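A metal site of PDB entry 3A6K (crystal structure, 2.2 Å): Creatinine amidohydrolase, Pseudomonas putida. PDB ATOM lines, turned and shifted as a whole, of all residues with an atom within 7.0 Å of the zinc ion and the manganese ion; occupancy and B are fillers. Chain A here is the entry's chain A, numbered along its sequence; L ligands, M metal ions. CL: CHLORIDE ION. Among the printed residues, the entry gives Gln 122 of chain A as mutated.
Of the 24 residues printed, 3 come within 4 Å of the manganese ion.
The nearest printed residue that does not touch the manganese ion is Gln 122 (4.1 Å).
The side-chain carboxylate (OE1) of Glu 183 sits at hydrogen-bond distance from the backbone NH (N) of Gly 179 (3.1 Å).
A ring nitrogen (ND1) of His 36 lies within hydrogen-bond range of the backbone carbonyl oxygen of Glu 34, at 2.9 Å.
The side-chain carboxylate (OE2) of Glu 34 is in hydrogen-bond range of the side-chain hydroxyl (OG) of Ser 74, at 3.1 Å.
A ring nitrogen (NE2) of His 120 sits close to the side-chain amide nitrogen (NE2) of Gln 122, at 3.4 Å.
NE2 of His 120 is in hydrogen-bond range of O of Tyr 72 (2.9 Å).
Three residues have an atom within 4 Å of the zinc ion: His 36, Asp 45 and Glu 183.
The nearest printed residue that does not touch the zinc ion is His 178 (4.1 Å).
The manganese ion is bound by the side-chain carboxylate of Glu 34, a ring nitrogen (ND1) of His 120, the side-chain carboxylate of Asp 45 and a chlorine (CL) of the ligand.
The manganese ion has four donor atoms within binding distance.
The zinc ion is bound by the side-chain carboxylate (OE2) of Glu 183 (2.0 Å), a ring nitrogen (NE2) of His 36 (2.1 Å) and the side-chain carboxylate (OD1) of Asp 45 (2.1 Å).
The zinc ion has three donor atoms within binding distance.
Slightly farther from the zinc ion lies the side-chain carboxylate (OE1) of Glu 183 (2.7 Å).
Slightly farther from the zinc ion lies a chlorine (CL) of the ligand (3.0 Å).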
ATOM      1  N   GLY A  31      -2.205   8.795 -13.959  1.00  0.00           N
ATOM      2  CA  GLY A  31      -2.787   7.838 -14.881  1.00  0.00           C
ATOM      3  C   GLY A  31      -2.253   6.420 -14.828  1.00  0.00           C
ATOM      4  O   GLY A  31      -2.006   5.881 -13.741  1.00  0.00           O
ATOM      5  N   ALA A  32      -2.081   5.824 -15.993  1.00  0.00           N
ATOM      6  CA  ALA A  32      -1.580   4.458 -16.095  1.00  0.00           C
ATOM      7  C   ALA A  32      -1.291   4.047 -17.536  1.00  0.00           C
ATOM      8  O   ALA A  32      -1.778   4.684 -18.481  1.00  0.00           O
ATOM      9  CB  ALA A  32      -2.595   3.484 -15.482  1.00  0.00           C
ATOM     10  N   GLU A  34      -2.172   1.165 -19.538  1.00  0.00           N
ATOM     11  CA  GLU A  34      -3.060   0.013 -19.454  1.00  0.00           C
ATOM     12  C   GLU A  34      -3.782  -0.307 -20.769  1.00  0.00           C
ATOM     13  O   GLU A  34      -4.118   0.589 -21.544  1.00  0.00           O
ATOM     14  CB  GLU A  34      -4.069   0.313 -18.347  1.00  0.00           C
ATOM     15  CG  GLU A  34      -5.057  -0.766 -18.016  1.00  0.00           C
ATOM     16  CD  GLU A  34      -6.095  -0.248 -17.038  1.00  0.00           C
ATOM     17  OE1 GLU A  34      -6.562   0.893 -17.240  1.00  0.00           O
ATOM     18  OE2 GLU A  34      -6.443  -0.967 -16.088  1.00  0.00           O
ATOM     19  N   GLN A  35      -4.033  -1.588 -21.011  1.00  0.00           N
ATOM     20  CA  GLN A  35      -4.721  -1.979 -22.228  1.00  0.00           C
ATOM     21  C   GLN A  35      -6.114  -1.375 -22.253  1.00  0.00           C
ATOM     22  O   GLN A  35      -6.789  -1.282 -21.231  1.00  0.00           O
ATOM     23  CB  GLN A  35      -4.792  -3.509 -22.366  1.00  0.00           C
ATOM     24  CG  GLN A  35      -5.651  -4.258 -21.358  1.00  0.00           C
ATOM     25  CD  GLN A  35      -7.141  -4.107 -21.617  1.00  0.00           C
ATOM     26  OE1 GLN A  35      -7.570  -3.940 -22.754  1.00  0.00           O
ATOM     27  NE2 GLN A  35      -7.935  -4.176 -20.548  1.00  0.00           N
ATOM     28  N   HIS A  36      -6.540  -0.931 -23.438  1.00  0.00           N
ATOM     29  CA  HIS A  36      -7.854  -0.340 -23.604  1.00  0.00           C
ATOM     30  C   HIS A  36      -8.587  -0.935 -24.800  1.00  0.00           C
ATOM     31  O   HIS A  36      -9.097  -0.206 -25.661  1.00  0.00           O
ATOM     32  CB  HIS A  36      -7.758   1.172 -23.741  1.00  0.00           C
ATOM     33  CG  HIS A  36      -7.754   1.883 -22.420  1.00  0.00           C
ATOM     34  ND1 HIS A  36      -6.695   1.824 -21.551  1.00  0.00           N
ATOM     35  CD2 HIS A  36      -8.714   2.607 -21.807  1.00  0.00           C
ATOM     36  CE1 HIS A  36      -7.003   2.481 -20.448  1.00  0.00           C
ATOM     37  NE2 HIS A  36      -8.229   2.967 -20.570  1.00  0.00           N
ATOM     38  N   MET A  40      -8.469   1.460 -28.730  1.00  0.00           N
ATOM     39  CA  MET A  40      -7.739   2.608 -28.187  1.00  0.00           C
ATOM     40  C   MET A  40      -6.336   2.297 -27.723  1.00  0.00           C
ATOM     41  O   MET A  40      -5.995   1.147 -27.422  1.00  0.00           O
ATOM     42  CB  MET A  40      -8.508   3.238 -27.016  1.00  0.00           C
ATOM     43  CG  MET A  40      -9.816   3.884 -27.378  1.00  0.00           C
ATOM     44  SD  MET A  40     -10.475   4.854 -26.011  1.00  0.00           S
ATOM     45  CE  MET A  40     -10.958   3.542 -24.892  1.00  0.00           C
ATOM     46  N   VAL A  44      -4.454   6.208 -22.383  1.00  0.00           N
ATOM     47  CA  VAL A  44      -5.717   6.916 -22.192  1.00  0.00           C
ATOM     48  C   VAL A  44      -5.860   7.541 -20.808  1.00  0.00           C
ATOM     49  O   VAL A  44      -6.225   8.707 -20.679  1.00  0.00           O
ATOM     50  CB  VAL A  44      -6.920   5.959 -22.416  1.00  0.00           C
ATOM     51  CG1 VAL A  44      -8.221   6.605 -21.950  1.00  0.00           C
ATOM     52  CG2 VAL A  44      -7.002   5.584 -23.898  1.00  0.00           C
ATOM     53  N   ASP A  45      -5.564   6.745 -19.772  1.00  0.00           N
ATOM     54  CA  ASP A  45      -5.675   7.213 -18.395  1.00  0.00           C
ATOM     55  C   ASP A  45      -4.738   8.345 -18.014  1.00  0.00           C
ATOM     56  O   ASP A  45      -4.898   8.947 -16.960  1.00  0.00           O
ATOM     57  CB  ASP A  45      -5.475   6.047 -17.432  1.00  0.00           C
ATOM     58  CG  ASP A  45      -6.577   5.031 -17.535  1.00  0.00           C
ATOM     59  OD1 ASP A  45      -7.489   5.248 -18.358  1.00  0.00           O
ATOM     60  OD2 ASP A  45      -6.535   4.013 -16.814  1.00  0.00           O
ATOM     61  N   LEU A  48      -6.502  11.616 -20.812  1.00  0.00           N
ATOM     62  CA  LEU A  48      -7.768  12.207 -20.383  1.00  0.00           C
ATOM     63  C   LEU A  48      -7.649  13.140 -19.176  1.00  0.00           C
ATOM     64  O   LEU A  48      -8.039  14.304 -19.250  1.00  0.00           O
ATOM     65  CB  LEU A  48      -8.806  11.106 -20.144  1.00  0.00           C
ATOM     66  CG  LEU A  48      -9.154  10.276 -21.395  1.00  0.00           C
ATOM     67  CD1 LEU A  48     -10.309   9.340 -21.097  1.00  0.00           C
ATOM     68  CD2 LEU A  48      -9.523  11.207 -22.536  1.00  0.00           C
ATOM     69  N   TYR A  72      -1.343   1.958 -10.370  1.00  0.00           N
ATOM     70  CA  TYR A  72      -1.512   0.685  -9.699  1.00  0.00           C
ATOM     71  C   TYR A  72      -2.066  -0.424 -10.591  1.00  0.00           C
ATOM     72  O   TYR A  72      -2.757  -0.153 -11.557  1.00  0.00           O
ATOM     73  CB  TYR A  72      -2.431   0.836  -8.474  1.00  0.00           C
ATOM     74  CG  TYR A  72      -2.430  -0.417  -7.638  1.00  0.00           C
ATOM     75  CD1 TYR A  72      -1.250  -0.913  -7.085  1.00  0.00           C
ATOM     76  CD2 TYR A  72      -3.598  -1.148  -7.457  1.00  0.00           C
ATOM     77  CE1 TYR A  72      -1.224  -2.101  -6.386  1.00  0.00           C
ATOM     78  CE2 TYR A  72      -3.576  -2.363  -6.749  1.00  0.00           C
ATOM     79  CZ  TYR A  72      -2.385  -2.824  -6.222  1.00  0.00           C
ATOM     80  OH  TYR A  72      -2.367  -4.031  -5.558  1.00  0.00           O
ATOM     81  N   SER A  74      -3.918  -3.395 -12.494  1.00  0.00           N
ATOM     82  CA  SER A  74      -5.290  -3.470 -12.975  1.00  0.00           C
ATOM     83  C   SER A  74      -6.065  -4.602 -12.295  1.00  0.00           C
ATOM     84  O   SER A  74      -5.529  -5.686 -12.071  1.00  0.00           O
ATOM     85  CB  SER A  74      -5.300  -3.696 -14.495  1.00  0.00           C
ATOM     86  OG  SER A  74      -6.624  -3.857 -14.963  1.00  0.00           O
ATOM     87  N   SER A  78     -12.439  -4.175 -12.805  1.00  0.00           N
ATOM     88  CA  SER A  78     -12.347  -2.731 -13.014  1.00  0.00           C
ATOM     89  C   SER A  78     -11.518  -2.316 -14.228  1.00  0.00           C
ATOM     90  O   SER A  78     -11.521  -1.141 -14.614  1.00  0.00           O
ATOM     91  CB  SER A  78     -11.785  -2.055 -11.764  1.00  0.00           C
ATOM     92  OG  SER A  78     -12.652  -2.220 -10.654  1.00  0.00           O
ATOM     93  N   GLY A  79     -10.805  -3.262 -14.830  1.00  0.00           N
ATOM     94  CA  GLY A  79      -9.986  -2.935 -15.973  1.00  0.00           C
ATOM     95  C   GLY A  79      -9.467  -4.146 -16.719  1.00  0.00           C
ATOM     96  O   GLY A  79      -8.387  -4.103 -17.324  1.00  0.00           O
ATOM     97  N   GLY A 119      -6.958   9.299 -13.225  1.00  0.00           N
ATOM     98  CA  GLY A 119      -7.600   8.830 -14.451  1.00  0.00           C
ATOM     99  C   GLY A 119      -7.702   7.316 -14.485  1.00  0.00           C
ATOM    100  O   GLY A 119      -8.285   6.748 -15.413  1.00  0.00           O
ATOM    101  N   HIS A 120      -7.142   6.664 -13.481  1.00  0.00           N
ATOM    102  CA  HIS A 120      -7.125   5.198 -13.381  1.00  0.00           C
ATOM    103  C   HIS A 120      -7.781   4.807 -12.059  1.00  0.00           C
ATOM    104  O   HIS A 120      -7.234   5.038 -10.981  1.00  0.00           O
ATOM    105  CB  HIS A 120      -5.666   4.715 -13.459  1.00  0.00           C
ATOM    106  CG  HIS A 120      -5.500   3.227 -13.381  1.00  0.00           C
ATOM    107  ND1 HIS A 120      -6.140   2.353 -14.237  1.00  0.00           N
ATOM    108  CD2 HIS A 120      -4.697   2.462 -12.607  1.00  0.00           C
ATOM    109  CE1 HIS A 120      -5.746   1.125 -13.990  1.00  0.00           C
ATOM    110  NE2 HIS A 120      -4.876   1.158 -12.998  1.00  0.00           N
ATOM    111  N   TYR A 121      -8.980   4.241 -12.166  1.00  0.00           N
ATOM    112  CA  TYR A 121      -9.799   3.807 -11.029  1.00  0.00           C
ATOM    113  C   TYR A 121      -9.042   3.184  -9.843  1.00  0.00           C
ATOM    114  O   TYR A 121      -9.284   3.527  -8.680  1.00  0.00           O
ATOM    115  CB  TYR A 121     -10.872   2.834 -11.518  1.00  0.00           C
ATOM    116  CG  TYR A 121     -11.830   2.357 -10.437  1.00  0.00           C
ATOM    117  CD1 TYR A 121     -12.675   3.258  -9.781  1.00  0.00           C
ATOM    118  CD2 TYR A 121     -11.857   1.018 -10.040  1.00  0.00           C
ATOM    119  CE1 TYR A 121     -13.532   2.836  -8.762  1.00  0.00           C
ATOM    120  CE2 TYR A 121     -12.712   0.587  -9.024  1.00  0.00           C
ATOM    121  CZ  TYR A 121     -13.541   1.496  -8.382  1.00  0.00           C
ATOM    122  OH  TYR A 121     -14.374   1.069  -7.367  1.00  0.00           O
ATOM    123  N   GLN A 122      -8.137   2.270 -10.145  1.00  0.00           N
ATOM    124  CA  GLN A 122      -7.353   1.554  -9.139  1.00  0.00           C
ATOM    125  C   GLN A 122      -6.316   2.359  -8.332  1.00  0.00           C
ATOM    126  O   GLN A 122      -5.856   1.894  -7.286  1.00  0.00           O
ATOM    127  CB  GLN A 122      -6.634   0.366  -9.790  1.00  0.00           C
ATOM    128  CG  GLN A 122      -7.540  -0.794 -10.220  1.00  0.00           C
ATOM    129  CD  GLN A 122      -8.171  -0.616 -11.603  1.00  0.00           C
ATOM    130  OE1 GLN A 122      -8.729  -1.555 -12.159  1.00  0.00           O
ATOM    131  NE2 GLN A 122      -8.082   0.594 -12.160  1.00  0.00           N
ATOM    132  N   ASN A 123      -5.952   3.550  -8.795  1.00  0.00           N
ATOM    133  CA  ASN A 123      -4.959   4.372  -8.093  1.00  0.00           C
ATOM    134  C   ASN A 123      -5.432   4.996  -6.800  1.00  0.00           C
ATOM    135  O   ASN A 123      -4.637   5.258  -5.903  1.00  0.00           O
ATOM    136  CB  ASN A 123      -4.467   5.526  -8.977  1.00  0.00           C
ATOM    137  CG  ASN A 123      -3.703   5.075 -10.180  1.00  0.00           C
ATOM    138  OD1 ASN A 123      -3.001   4.059 -10.151  1.00  0.00           O
ATOM    139  ND2 ASN A 123      -3.800   5.843 -11.254  1.00  0.00           N
ATOM    140  N   TYR A 153     -12.060  12.610 -12.371  1.00  0.00           N
ATOM    141  CA  TYR A 153     -12.895  13.436 -13.222  1.00  0.00           C
ATOM    142  C   TYR A 153     -14.273  12.876 -13.605  1.00  0.00           C
ATOM    143  O   TYR A 153     -15.225  13.628 -13.753  1.00  0.00           O
ATOM    144  CB  TYR A 153     -12.120  13.834 -14.492  1.00  0.00           C
ATOM    145  CG  TYR A 153     -11.883  12.703 -15.471  1.00  0.00           C
ATOM    146  CD1 TYR A 153     -12.900  12.290 -16.334  1.00  0.00           C
ATOM    147  CD2 TYR A 153     -10.671  12.030 -15.509  1.00  0.00           C
ATOM    148  CE1 TYR A 153     -12.704  11.237 -17.207  1.00  0.00           C
ATOM    149  CE2 TYR A 153     -10.472  10.959 -16.390  1.00  0.00           C
ATOM    150  CZ  TYR A 153     -11.498  10.579 -17.228  1.00  0.00           C
ATOM    151  OH  TYR A 153     -11.339   9.527 -18.092  1.00  0.00           O
ATOM    152  N   TRP A 154     -14.373  11.561 -13.741  1.00  0.00           N
ATOM    153  CA  TRP A 154     -15.650  10.966 -14.135  1.00  0.00           C
ATOM    154  C   TRP A 154     -16.747  11.088 -13.083  1.00  0.00           C
ATOM    155  O   TRP A 154     -17.937  10.917 -13.380  1.00  0.00           O
ATOM    156  CB  TRP A 154     -15.459   9.496 -14.515  1.00  0.00           C
ATOM    157  CG  TRP A 154     -14.871   8.648 -13.455  1.00  0.00           C
ATOM    158  CD1 TRP A 154     -15.476   8.212 -12.313  1.00  0.00           C
ATOM    159  CD2 TRP A 154     -13.537   8.126 -13.414  1.00  0.00           C
ATOM    160  NE1 TRP A 154     -14.607   7.459 -11.567  1.00  0.00           N
ATOM    161  CE2 TRP A 154     -13.404   7.386 -12.214  1.00  0.00           C
ATOM    162  CE3 TRP A 154     -12.425   8.212 -14.281  1.00  0.00           C
ATOM    163  CZ2 TRP A 154     -12.215   6.743 -11.852  1.00  0.00           C
ATOM    164  CZ3 TRP A 154     -11.244   7.570 -13.923  1.00  0.00           C
ATOM    165  CH2 TRP A 154     -11.146   6.844 -12.718  1.00  0.00           C
ATOM    166  N   GLU A 177     -17.194   0.201 -17.167  1.00  0.00           N
ATOM    167  CA  GLU A 177     -16.948   1.299 -18.087  1.00  0.00           C
ATOM    168  C   GLU A 177     -15.480   1.419 -18.501  1.00  0.00           C
ATOM    169  O   GLU A 177     -15.003   2.520 -18.795  1.00  0.00           O
ATOM    170  CB  GLU A 177     -17.450   2.597 -17.457  1.00  0.00           C
ATOM    171  CG  GLU A 177     -17.578   3.770 -18.435  1.00  0.00           C
ATOM    172  CD  GLU A 177     -18.429   3.451 -19.647  1.00  0.00           C
ATOM    173  OE1 GLU A 177     -19.604   3.037 -19.488  1.00  0.00           O
ATOM    174  OE2 GLU A 177     -17.921   3.612 -20.778  1.00  0.00           O
ATOM    175  N   HIS A 178     -14.765   0.299 -18.532  1.00  0.00           N
ATOM    176  CA  HIS A 178     -13.358   0.305 -18.934  1.00  0.00           C
ATOM    177  C   HIS A 178     -13.263   0.157 -20.442  1.00  0.00           C
ATOM    178  O   HIS A 178     -13.518  -0.927 -20.981  1.00  0.00           O
ATOM    179  CB  HIS A 178     -12.591  -0.845 -18.276  1.00  0.00           C
ATOM    180  CG  HIS A 178     -11.150  -0.930 -18.686  1.00  0.00           C
ATOM    181  ND1 HIS A 178     -10.211  -0.013 -18.269  1.00  0.00           N
ATOM    182  CD2 HIS A 178     -10.503  -1.797 -19.491  1.00  0.00           C
ATOM    183  CE1 HIS A 178      -9.034  -0.303 -18.810  1.00  0.00           C
ATOM    184  NE2 HIS A 178      -9.184  -1.380 -19.553  1.00  0.00           N
ATOM    185  N   GLY A 179     -12.877   1.228 -21.125  1.00  0.00           N
ATOM    186  CA  GLY A 179     -12.761   1.179 -22.574  1.00  0.00           C
ATOM    187  C   GLY A 179     -14.119   1.244 -23.241  1.00  0.00           C
ATOM    188  O   GLY A 179     -14.256   1.027 -24.451  1.00  0.00           O
ATOM    189  N   GLU A 183     -14.948   6.589 -21.935  1.00  0.00           N
ATOM    190  CA  GLU A 183     -13.568   6.909 -22.308  1.00  0.00           C
ATOM    191  C   GLU A 183     -13.388   7.077 -23.800  1.00  0.00           C
ATOM    192  O   GLU A 183     -12.660   7.964 -24.242  1.00  0.00           O
ATOM    193  CB  GLU A 183     -12.612   5.841 -21.817  1.00  0.00           C
ATOM    194  CG  GLU A 183     -12.351   5.871 -20.339  1.00  0.00           C
ATOM    195  CD  GLU A 183     -11.227   4.935 -19.962  1.00  0.00           C
ATOM    196  OE1 GLU A 183     -11.342   3.725 -20.242  1.00  0.00           O
ATOM    197  OE2 GLU A 183     -10.223   5.415 -19.381  1.00  0.00           O
HETATM  198 CL    CL L   1     -10.113   3.160 -16.135  1.00  0.00          CL
HETATM  199 ZN    ZN M   1      -9.042   3.880 -18.854  1.00  0.00          ZN
HETATM  200 MN    MN M   2      -7.558   2.274 -15.900  1.00  0.00          MN
